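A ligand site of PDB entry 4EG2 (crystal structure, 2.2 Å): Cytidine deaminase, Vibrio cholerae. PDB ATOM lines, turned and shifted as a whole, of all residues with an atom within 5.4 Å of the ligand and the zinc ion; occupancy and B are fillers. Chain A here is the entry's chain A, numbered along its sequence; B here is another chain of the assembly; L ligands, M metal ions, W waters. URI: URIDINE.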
ATOM      1  N   ALA A  69     -16.902 -26.344 -17.734  1.00  0.00           N
ATOM      2  CA  ALA A  69     -17.705 -25.828 -18.829  1.00  0.00           C
ATOM      3  C   ALA A  69     -18.866 -24.970 -18.336  1.00  0.00           C
ATOM      4  O   ALA A  69     -20.033 -25.374 -18.456  1.00  0.00           O
ATOM      5  CB  ALA A  69     -18.204 -26.992 -19.656  1.00  0.00           C
ATOM      6  N   SER A  72     -21.121 -23.741 -21.726  1.00  0.00           N
ATOM      7  CA  SER A  72     -21.924 -24.761 -22.387  1.00  0.00           C
ATOM      8  C   SER A  72     -22.545 -25.821 -21.480  1.00  0.00           C
ATOM      9  O   SER A  72     -23.571 -26.418 -21.851  1.00  0.00           O
ATOM     10  CB  SER A  72     -21.047 -25.525 -23.359  1.00  0.00           C
ATOM     11  OG  SER A  72     -20.128 -26.355 -22.632  1.00  0.00           O
ATOM     12  N   PHE A  74     -21.480 -28.583 -21.135  1.00  0.00           N
ATOM     13  CA  PHE A  74     -21.338 -29.777 -21.986  1.00  0.00           C
ATOM     14  C   PHE A  74     -19.955 -30.327 -21.630  1.00  0.00           C
ATOM     15  O   PHE A  74     -18.953 -29.733 -21.979  1.00  0.00           O
ATOM     16  CB  PHE A  74     -21.435 -29.325 -23.429  1.00  0.00           C
ATOM     17  CG  PHE A  74     -21.315 -30.420 -24.417  1.00  0.00           C
ATOM     18  CD1 PHE A  74     -22.376 -31.285 -24.637  1.00  0.00           C
ATOM     19  CD2 PHE A  74     -20.172 -30.559 -25.165  1.00  0.00           C
ATOM     20  CE1 PHE A  74     -22.275 -32.289 -25.543  1.00  0.00           C
ATOM     21  CE2 PHE A  74     -20.070 -31.560 -26.085  1.00  0.00           C
ATOM     22  CZ  PHE A  74     -21.130 -32.440 -26.272  1.00  0.00           C
ATOM     23  N   VAL A  76     -16.845 -32.769 -21.692  1.00  0.00           N
ATOM     24  CA  VAL A  76     -16.106 -33.642 -22.577  1.00  0.00           C
ATOM     25  C   VAL A  76     -14.846 -34.109 -21.881  1.00  0.00           C
ATOM     26  O   VAL A  76     -14.121 -33.329 -21.273  1.00  0.00           O
ATOM     27  CB  VAL A  76     -15.760 -32.894 -23.881  1.00  0.00           C
ATOM     28  CG1 VAL A  76     -15.179 -33.836 -24.914  1.00  0.00           C
ATOM     29  CG2 VAL A  76     -17.018 -32.192 -24.453  1.00  0.00           C
ATOM     30  N   ASN A  92     -12.485 -30.462 -21.116  1.00  0.00           N
ATOM     31  CA  ASN A  92     -12.605 -29.165 -21.754  1.00  0.00           C
ATOM     32  C   ASN A  92     -12.637 -28.038 -20.718  1.00  0.00           C
ATOM     33  O   ASN A  92     -12.995 -28.280 -19.571  1.00  0.00           O
ATOM     34  CB  ASN A  92     -13.812 -29.111 -22.720  1.00  0.00           C
ATOM     35  CG  ASN A  92     -15.134 -29.430 -22.052  1.00  0.00           C
ATOM     36  OD1 ASN A  92     -15.217 -30.333 -21.211  1.00  0.00           O
ATOM     37  ND2 ASN A  92     -16.197 -28.721 -22.475  1.00  0.00           N
ATOM     38  N   MET A  93     -12.209 -26.862 -21.113  1.00  0.00           N
ATOM     39  CA  MET A  93     -12.202 -25.671 -20.224  1.00  0.00           C
ATOM     40  C   MET A  93     -12.742 -24.473 -20.997  1.00  0.00           C
ATOM     41  O   MET A  93     -12.310 -24.219 -22.132  1.00  0.00           O
ATOM     42  CB  MET A  93     -10.807 -25.314 -19.744  1.00  0.00           C
ATOM     43  CG  MET A  93     -10.019 -26.454 -19.206  1.00  0.00           C
ATOM     44  SD  MET A  93      -8.270 -25.898 -18.490  1.00  0.00           S
ATOM     45  CE  MET A  93      -7.572 -24.806 -19.947  1.00  0.00           C
ATOM     46  N   GLU A  94     -13.660 -23.753 -20.382  1.00  0.00           N
ATOM     47  CA  GLU A  94     -14.279 -22.565 -20.982  1.00  0.00           C
ATOM     48  C   GLU A  94     -14.126 -21.396 -20.009  1.00  0.00           C
ATOM     49  O   GLU A  94     -14.152 -21.587 -18.781  1.00  0.00           O
ATOM     50  CB  GLU A  94     -15.762 -22.814 -21.215  1.00  0.00           C
ATOM     51  CG  GLU A  94     -16.047 -24.030 -22.091  1.00  0.00           C
ATOM     52  CD  GLU A  94     -17.519 -24.405 -22.090  1.00  0.00           C
ATOM     53  OE1 GLU A  94     -18.284 -23.884 -21.246  1.00  0.00           O
ATOM     54  OE2 GLU A  94     -17.902 -25.247 -22.919  1.00  0.00           O
ATOM     55  N   THR A 103     -10.985 -20.908 -25.408  1.00  0.00           N
ATOM     56  CA  THR A 103     -11.528 -22.228 -25.022  1.00  0.00           C
ATOM     57  C   THR A 103     -10.523 -23.346 -25.250  1.00  0.00           C
ATOM     58  O   THR A 103      -9.748 -23.303 -26.204  1.00  0.00           O
ATOM     59  CB  THR A 103     -12.797 -22.569 -25.852  1.00  0.00           C
ATOM     60  OG1 THR A 103     -13.740 -21.482 -25.773  1.00  0.00           O
ATOM     61  CG2 THR A 103     -13.464 -23.886 -25.376  1.00  0.00           C
ATOM     62  N   VAL A 104     -10.506 -24.339 -24.355  1.00  0.00           N
ATOM     63  CA  VAL A 104      -9.638 -25.503 -24.516  1.00  0.00           C
ATOM     64  C   VAL A 104     -10.512 -26.754 -24.599  1.00  0.00           C
ATOM     65  O   VAL A 104     -11.377 -26.972 -23.762  1.00  0.00           O
ATOM     66  CB  VAL A 104      -8.584 -25.629 -23.403  1.00  0.00           C
ATOM     67  CG1 VAL A 104      -7.755 -26.904 -23.569  1.00  0.00           C
ATOM     68  CG2 VAL A 104      -7.671 -24.406 -23.397  1.00  0.00           C
ATOM     69  N   HIS A 105     -10.303 -27.538 -25.639  1.00  0.00           N
ATOM     70  CA  HIS A 105     -11.041 -28.775 -25.850  1.00  0.00           C
ATOM     71  C   HIS A 105     -10.397 -29.913 -25.107  1.00  0.00           C
ATOM     72  O   HIS A 105      -9.187 -29.909 -24.914  1.00  0.00           O
ATOM     73  CB  HIS A 105     -11.054 -29.129 -27.336  1.00  0.00           C
ATOM     74  CG  HIS A 105     -11.882 -28.199 -28.172  1.00  0.00           C
ATOM     75  ND1 HIS A 105     -12.928 -28.633 -28.950  1.00  0.00           N
ATOM     76  CD2 HIS A 105     -11.821 -26.851 -28.325  1.00  0.00           C
ATOM     77  CE1 HIS A 105     -13.476 -27.595 -29.562  1.00  0.00           C
ATOM     78  NE2 HIS A 105     -12.828 -26.500 -29.194  1.00  0.00           N
ATOM     79  N   ALA A 106     -11.210 -30.900 -24.704  1.00  0.00           N
ATOM     80  CA  ALA A 106     -10.717 -32.075 -23.982  1.00  0.00           C
ATOM     81  C   ALA A 106      -9.522 -32.668 -24.700  1.00  0.00           C
ATOM     82  O   ALA A 106      -8.518 -32.983 -24.066  1.00  0.00           O
ATOM     83  CB  ALA A 106     -11.841 -33.154 -23.817  1.00  0.00           C
ATOM     84  N   GLU A 107      -9.626 -32.798 -26.010  1.00  0.00           N
ATOM     85  CA  GLU A 107      -8.539 -33.369 -26.816  1.00  0.00           C
ATOM     86  C   GLU A 107      -7.239 -32.587 -26.665  1.00  0.00           C
ATOM     87  O   GLU A 107      -6.157 -33.174 -26.444  1.00  0.00           O
ATOM     88  CB  GLU A 107      -8.919 -33.444 -28.290  1.00  0.00           C
ATOM     89  CG  GLU A 107     -10.080 -34.403 -28.636  1.00  0.00           C
ATOM     90  CD  GLU A 107     -11.506 -33.801 -28.487  1.00  0.00           C
ATOM     91  OE1 GLU A 107     -11.692 -32.809 -27.764  1.00  0.00           O
ATOM     92  OE2 GLU A 107     -12.438 -34.324 -29.129  1.00  0.00           O
ATOM     93  N   PHE A 129     -16.991 -37.555 -27.075  1.00  0.00           N
ATOM     94  CA  PHE A 129     -17.744 -37.274 -28.302  1.00  0.00           C
ATOM     95  C   PHE A 129     -16.797 -37.194 -29.513  1.00  0.00           C
ATOM     96  O   PHE A 129     -15.585 -36.985 -29.345  1.00  0.00           O
ATOM     97  CB  PHE A 129     -18.478 -35.934 -28.188  1.00  0.00           C
ATOM     98  CG  PHE A 129     -19.360 -35.823 -26.982  1.00  0.00           C
ATOM     99  CD1 PHE A 129     -20.688 -36.257 -27.019  1.00  0.00           C
ATOM    100  CD2 PHE A 129     -18.883 -35.280 -25.797  1.00  0.00           C
ATOM    101  CE1 PHE A 129     -21.513 -36.159 -25.899  1.00  0.00           C
ATOM    102  CE2 PHE A 129     -19.696 -35.185 -24.669  1.00  0.00           C
ATOM    103  CZ  PHE A 129     -21.010 -35.614 -24.725  1.00  0.00           C
ATOM    104  N   SER A 130     -17.335 -37.350 -30.725  1.00  0.00           N
ATOM    105  CA  SER A 130     -16.538 -37.270 -31.961  1.00  0.00           C
ATOM    106  C   SER A 130     -15.841 -35.921 -32.019  1.00  0.00           C
ATOM    107  O   SER A 130     -16.465 -34.891 -31.749  1.00  0.00           O
ATOM    108  CB  SER A 130     -17.389 -37.428 -33.217  1.00  0.00           C
ATOM    109  OG  SER A 130     -16.583 -37.357 -34.381  1.00  0.00           O
ATOM    110  N   PRO A 131     -14.545 -35.924 -32.365  1.00  0.00           N
ATOM    111  CA  PRO A 131     -13.771 -34.691 -32.358  1.00  0.00           C
ATOM    112  C   PRO A 131     -14.201 -33.705 -33.442  1.00  0.00           C
ATOM    113  O   PRO A 131     -14.424 -34.112 -34.583  1.00  0.00           O
ATOM    114  CB  PRO A 131     -12.332 -35.186 -32.615  1.00  0.00           C
ATOM    115  CG  PRO A 131     -12.491 -36.429 -33.366  1.00  0.00           C
ATOM    116  CD  PRO A 131     -13.748 -37.067 -32.831  1.00  0.00           C
ATOM    117  N   CYS A 132     -14.308 -32.427 -33.066  1.00  0.00           N
ATOM    118  CA  CYS A 132     -14.663 -31.360 -33.995  1.00  0.00           C
ATOM    119  C   CYS A 132     -13.466 -31.107 -34.931  1.00  0.00           C
ATOM    120  O   CYS A 132     -12.382 -31.673 -34.718  1.00  0.00           O
ATOM    121  CB  CYS A 132     -15.039 -30.084 -33.259  1.00  0.00           C
ATOM    122  SG  CYS A 132     -13.654 -29.213 -32.536  1.00  0.00           S
ATOM    123  N   GLY A 133     -13.669 -30.282 -35.952  1.00  0.00           N
ATOM    124  CA  GLY A 133     -12.633 -29.995 -36.949  1.00  0.00           C
ATOM    125  C   GLY A 133     -11.408 -29.304 -36.382  1.00  0.00           C
ATOM    126  O   GLY A 133     -10.281 -29.526 -36.807  1.00  0.00           O
ATOM    127  N   HIS A 134     -11.651 -28.435 -35.404  1.00  0.00           N
ATOM    128  CA  HIS A 134     -10.584 -27.719 -34.715  1.00  0.00           C
ATOM    129  C   HIS A 134      -9.635 -28.736 -34.029  1.00  0.00           C
ATOM    130  O   HIS A 134      -8.415 -28.633 -34.170  1.00  0.00           O
ATOM    131  CB  HIS A 134     -11.240 -26.730 -33.737  1.00  0.00           C
ATOM    132  CG  HIS A 134     -10.326 -26.155 -32.713  1.00  0.00           C
ATOM    133  ND1 HIS A 134      -9.646 -24.973 -32.900  1.00  0.00           N
ATOM    134  CD2 HIS A 134     -10.035 -26.562 -31.456  1.00  0.00           C
ATOM    135  CE1 HIS A 134      -8.953 -24.699 -31.808  1.00  0.00           C
ATOM    136  NE2 HIS A 134      -9.175 -25.636 -30.918  1.00  0.00           N
ATOM    137  N   CYS A 135     -10.202 -29.743 -33.346  1.00  0.00           N
ATOM    138  CA  CYS A 135      -9.379 -30.779 -32.687  1.00  0.00           C
ATOM    139  C   CYS A 135      -8.708 -31.668 -33.680  1.00  0.00           C
ATOM    140  O   CYS A 135      -7.562 -32.052 -33.484  1.00  0.00           O
ATOM    141  CB  CYS A 135     -10.201 -31.646 -31.743  1.00  0.00           C
ATOM    142  SG  CYS A 135     -10.718 -30.787 -30.291  1.00  0.00           S
ATOM    143  N   PHE B 168     -19.089 -32.995 -35.574  1.00  0.00           N
ATOM    144  CA  PHE B 168     -19.579 -32.395 -34.381  1.00  0.00           C
ATOM    145  C   PHE B 168     -20.133 -31.078 -34.895  1.00  0.00           C
ATOM    146  O   PHE B 168     -19.576 -30.497 -35.815  1.00  0.00           O
ATOM    147  CB  PHE B 168     -18.460 -32.145 -33.379  1.00  0.00           C
ATOM    148  CG  PHE B 168     -18.877 -31.365 -32.195  1.00  0.00           C
ATOM    149  CD1 PHE B 168     -18.868 -29.992 -32.215  1.00  0.00           C
ATOM    150  CD2 PHE B 168     -19.308 -32.001 -31.047  1.00  0.00           C
ATOM    151  CE1 PHE B 168     -19.277 -29.268 -31.111  1.00  0.00           C
ATOM    152  CE2 PHE B 168     -19.711 -31.263 -29.946  1.00  0.00           C
ATOM    153  CZ  PHE B 168     -19.685 -29.910 -29.985  1.00  0.00           C
ATOM    154  N   LEU B 173     -25.225 -29.972 -29.556  1.00  0.00           N
ATOM    155  CA  LEU B 173     -25.583 -29.045 -28.472  1.00  0.00           C
ATOM    156  C   LEU B 173     -27.112 -28.791 -28.438  1.00  0.00           C
ATOM    157  O   LEU B 173     -27.585 -27.878 -27.770  1.00  0.00           O
ATOM    158  CB  LEU B 173     -24.803 -27.739 -28.598  1.00  0.00           C
ATOM    159  CG  LEU B 173     -23.283 -27.906 -28.491  1.00  0.00           C
ATOM    160  CD1 LEU B 173     -22.559 -26.570 -28.653  1.00  0.00           C
ATOM    161  CD2 LEU B 173     -22.907 -28.581 -27.165  1.00  0.00           C
ATOM    162  N   ALA B 235     -20.471 -23.766 -32.843  1.00  0.00           N
ATOM    163  CA  ALA B 235     -20.705 -24.762 -31.779  1.00  0.00           C
ATOM    164  C   ALA B 235     -19.399 -25.331 -31.195  1.00  0.00           C
ATOM    165  O   ALA B 235     -19.372 -25.730 -30.047  1.00  0.00           O
ATOM    166  CB  ALA B 235     -21.603 -25.875 -32.248  1.00  0.00           C
ATOM    167  N   ALA B 236     -18.343 -25.363 -31.996  1.00  0.00           N
ATOM    168  CA  ALA B 236     -17.038 -25.842 -31.520  1.00  0.00           C
ATOM    169  C   ALA B 236     -16.302 -24.742 -30.749  1.00  0.00           C
ATOM    170  O   ALA B 236     -15.205 -24.967 -30.257  1.00  0.00           O
ATOM    171  CB  ALA B 236     -16.225 -26.307 -32.653  1.00  0.00           C
ATOM    172  N   PHE B 237     -16.903 -23.566 -30.665  1.00  0.00           N
ATOM    173  CA  PHE B 237     -16.370 -22.415 -29.926  1.00  0.00           C
ATOM    174  C   PHE B 237     -15.171 -21.706 -30.581  1.00  0.00           C
ATOM    175  O   PHE B 237     -15.297 -20.563 -31.034  1.00  0.00           O
ATOM    176  CB  PHE B 237     -16.078 -22.801 -28.463  1.00  0.00           C
ATOM    177  CG  PHE B 237     -17.306 -22.825 -27.571  1.00  0.00           C
ATOM    178  CD1 PHE B 237     -18.546 -23.199 -28.053  1.00  0.00           C
ATOM    179  CD2 PHE B 237     -17.200 -22.521 -26.221  1.00  0.00           C
ATOM    180  CE1 PHE B 237     -19.672 -23.202 -27.225  1.00  0.00           C
ATOM    181  CE2 PHE B 237     -18.310 -22.559 -25.378  1.00  0.00           C
ATOM    182  CZ  PHE B 237     -19.541 -22.896 -25.886  1.00  0.00           C
ATOM    183  N   ASN B 238     -14.021 -22.343 -30.661  1.00  0.00           N
ATOM    184  CA  ASN B 238     -12.846 -21.680 -31.258  1.00  0.00           C
ATOM    185  C   ASN B 238     -13.047 -21.176 -32.699  1.00  0.00           C
ATOM    186  O   ASN B 238     -12.607 -20.078 -33.011  1.00  0.00           O
ATOM    187  CB  ASN B 238     -11.602 -22.545 -31.131  1.00  0.00           C
ATOM    188  CG  ASN B 238     -11.370 -22.972 -29.709  1.00  0.00           C
ATOM    189  OD1 ASN B 238     -12.195 -23.711 -29.159  1.00  0.00           O
ATOM    190  ND2 ASN B 238     -10.279 -22.519 -29.089  1.00  0.00           N
HETATM  191  N1  URI L   1     -15.544 -29.704 -27.030  1.00  0.00           N
HETATM  192  C2  URI L   1     -14.458 -30.541 -26.795  1.00  0.00           C
HETATM  193  N3  URI L   1     -14.131 -31.374 -27.843  1.00  0.00           N
HETATM  194  C4  URI L   1     -14.762 -31.450 -29.072  1.00  0.00           C
HETATM  195  C5  URI L   1     -15.878 -30.549 -29.256  1.00  0.00           C
HETATM  196  C6  URI L   1     -16.213 -29.722 -28.249  1.00  0.00           C
HETATM  197  O2  URI L   1     -13.834 -30.560 -25.762  1.00  0.00           O
HETATM  198  O4  URI L   1     -14.341 -32.233 -29.925  1.00  0.00           O
HETATM  199  C1' URI L   1     -15.988 -28.761 -26.018  1.00  0.00           C
HETATM  200  C2' URI L   1     -15.508 -27.350 -26.335  1.00  0.00           C
HETATM  201  C3' URI L   1     -16.534 -26.509 -25.602  1.00  0.00           C
HETATM  202  C4' URI L   1     -17.820 -27.315 -25.795  1.00  0.00           C
HETATM  203  O2' URI L   1     -14.179 -27.189 -25.923  1.00  0.00           O
HETATM  204  O3' URI L   1     -16.229 -26.360 -24.235  1.00  0.00           O
HETATM  205  O4' URI L   1     -17.395 -28.666 -26.073  1.00  0.00           O
HETATM  206  C5' URI L   1     -18.725 -26.840 -26.905  1.00  0.00           C
HETATM  207  O5' URI L   1     -18.075 -26.970 -28.150  1.00  0.00           O
HETATM  208 ZN    ZN M   1     -12.693 -30.145 -30.762  1.00  0.00          ZN
HETATM  209  O   HOH W   1     -15.044 -34.414 -28.562  1.00  0.00           O
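The backbone NH (N) of His 134 lies close to the side-chain sulfur (SG) of Cys 132 (3.6 Å). O of Ala 236 of chain B sits at hydrogen-bond distance from NE2 of His 105. O of Thr 103 lies within hydrogen-bond range of ND2 of Asn 238 of chain B. O of Val 104 lies within hydrogen-bond range of N of Met 93. The side-chain amide oxygen of Asn 238 of chain B lies close to the backbone carbonyl oxygen of Ala 236 of chain B (3.4 Å). NE2 of His 105 sits at hydrogen-bond distance from OD1 of Asn 238 of chain B (2.9 Å). ND2 of Asn 92 sits at hydrogen-bond distance from O of Phe 74 (3.0 Å). The side-chain carboxylate (OE2) of Glu 94 is in hydrogen-bond range of the side-chain hydroxyl (OG) of Ser 72, at 2.5 Å.
SG of Cys 135 is bound to the zinc ion (2.1 Å). SG of Cys 132 binds the zinc ion, at 2.2 Å. The zinc ion is bound by ND1 of His 105. The zinc ion has three donor atoms within binding distance. Slightly farther from the zinc ion lies an oxygen (O4) of the ligand (2.8 Å).
Residues that only touch the ligand: Thr 103, Phe 74, Pro 131, Val 104, Val 76, Ala 236 of chain B, Phe 237 of chain B, Phe 168 of chain B and Ser 130. Hydrophobic or aromatic side chains that line the ligand: Phe 74, Val 76, His 105, Ala 106, Phe 168 of chain B and Phe 237 of chain B. Of the 25 residues printed, 17 come within 4 Å of the ligand.
N3 of the ligand lies close to ND1 of His 105, at 3.2 Å. An oxygen (O4) of the ligand is in hydrogen-bond range of the backbone NH (N) of Cys 132 (3.1 Å). A nitrogen (N3) of the ligand is in hydrogen-bond range of the side-chain carboxylate of Glu 107. O3' of the ligand is in hydrogen-bond range of ND2 of Asn 92. The backbone NH of Ala 106 lies within hydrogen-bond range of an oxygen (O2) of the ligand (2.8 Å). An oxygen (O3') of the ligand lies within hydrogen-bond range of the side-chain carboxylate (OE2) of Glu 94 (2.4 Å). An oxygen (O5') of the ligand is in hydrogen-bond range of the backbone carbonyl oxygen (O) of Ala 235 of chain B (2.6 Å).
Of the 25 residues printed, 3 come within 4 Å of the zinc ion. Along chain A the residues within 4 Å of the zinc ion span positions 105 to 135. The nearest printed residue that does not touch the zinc ion is Glu 107 (4.1 Å).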
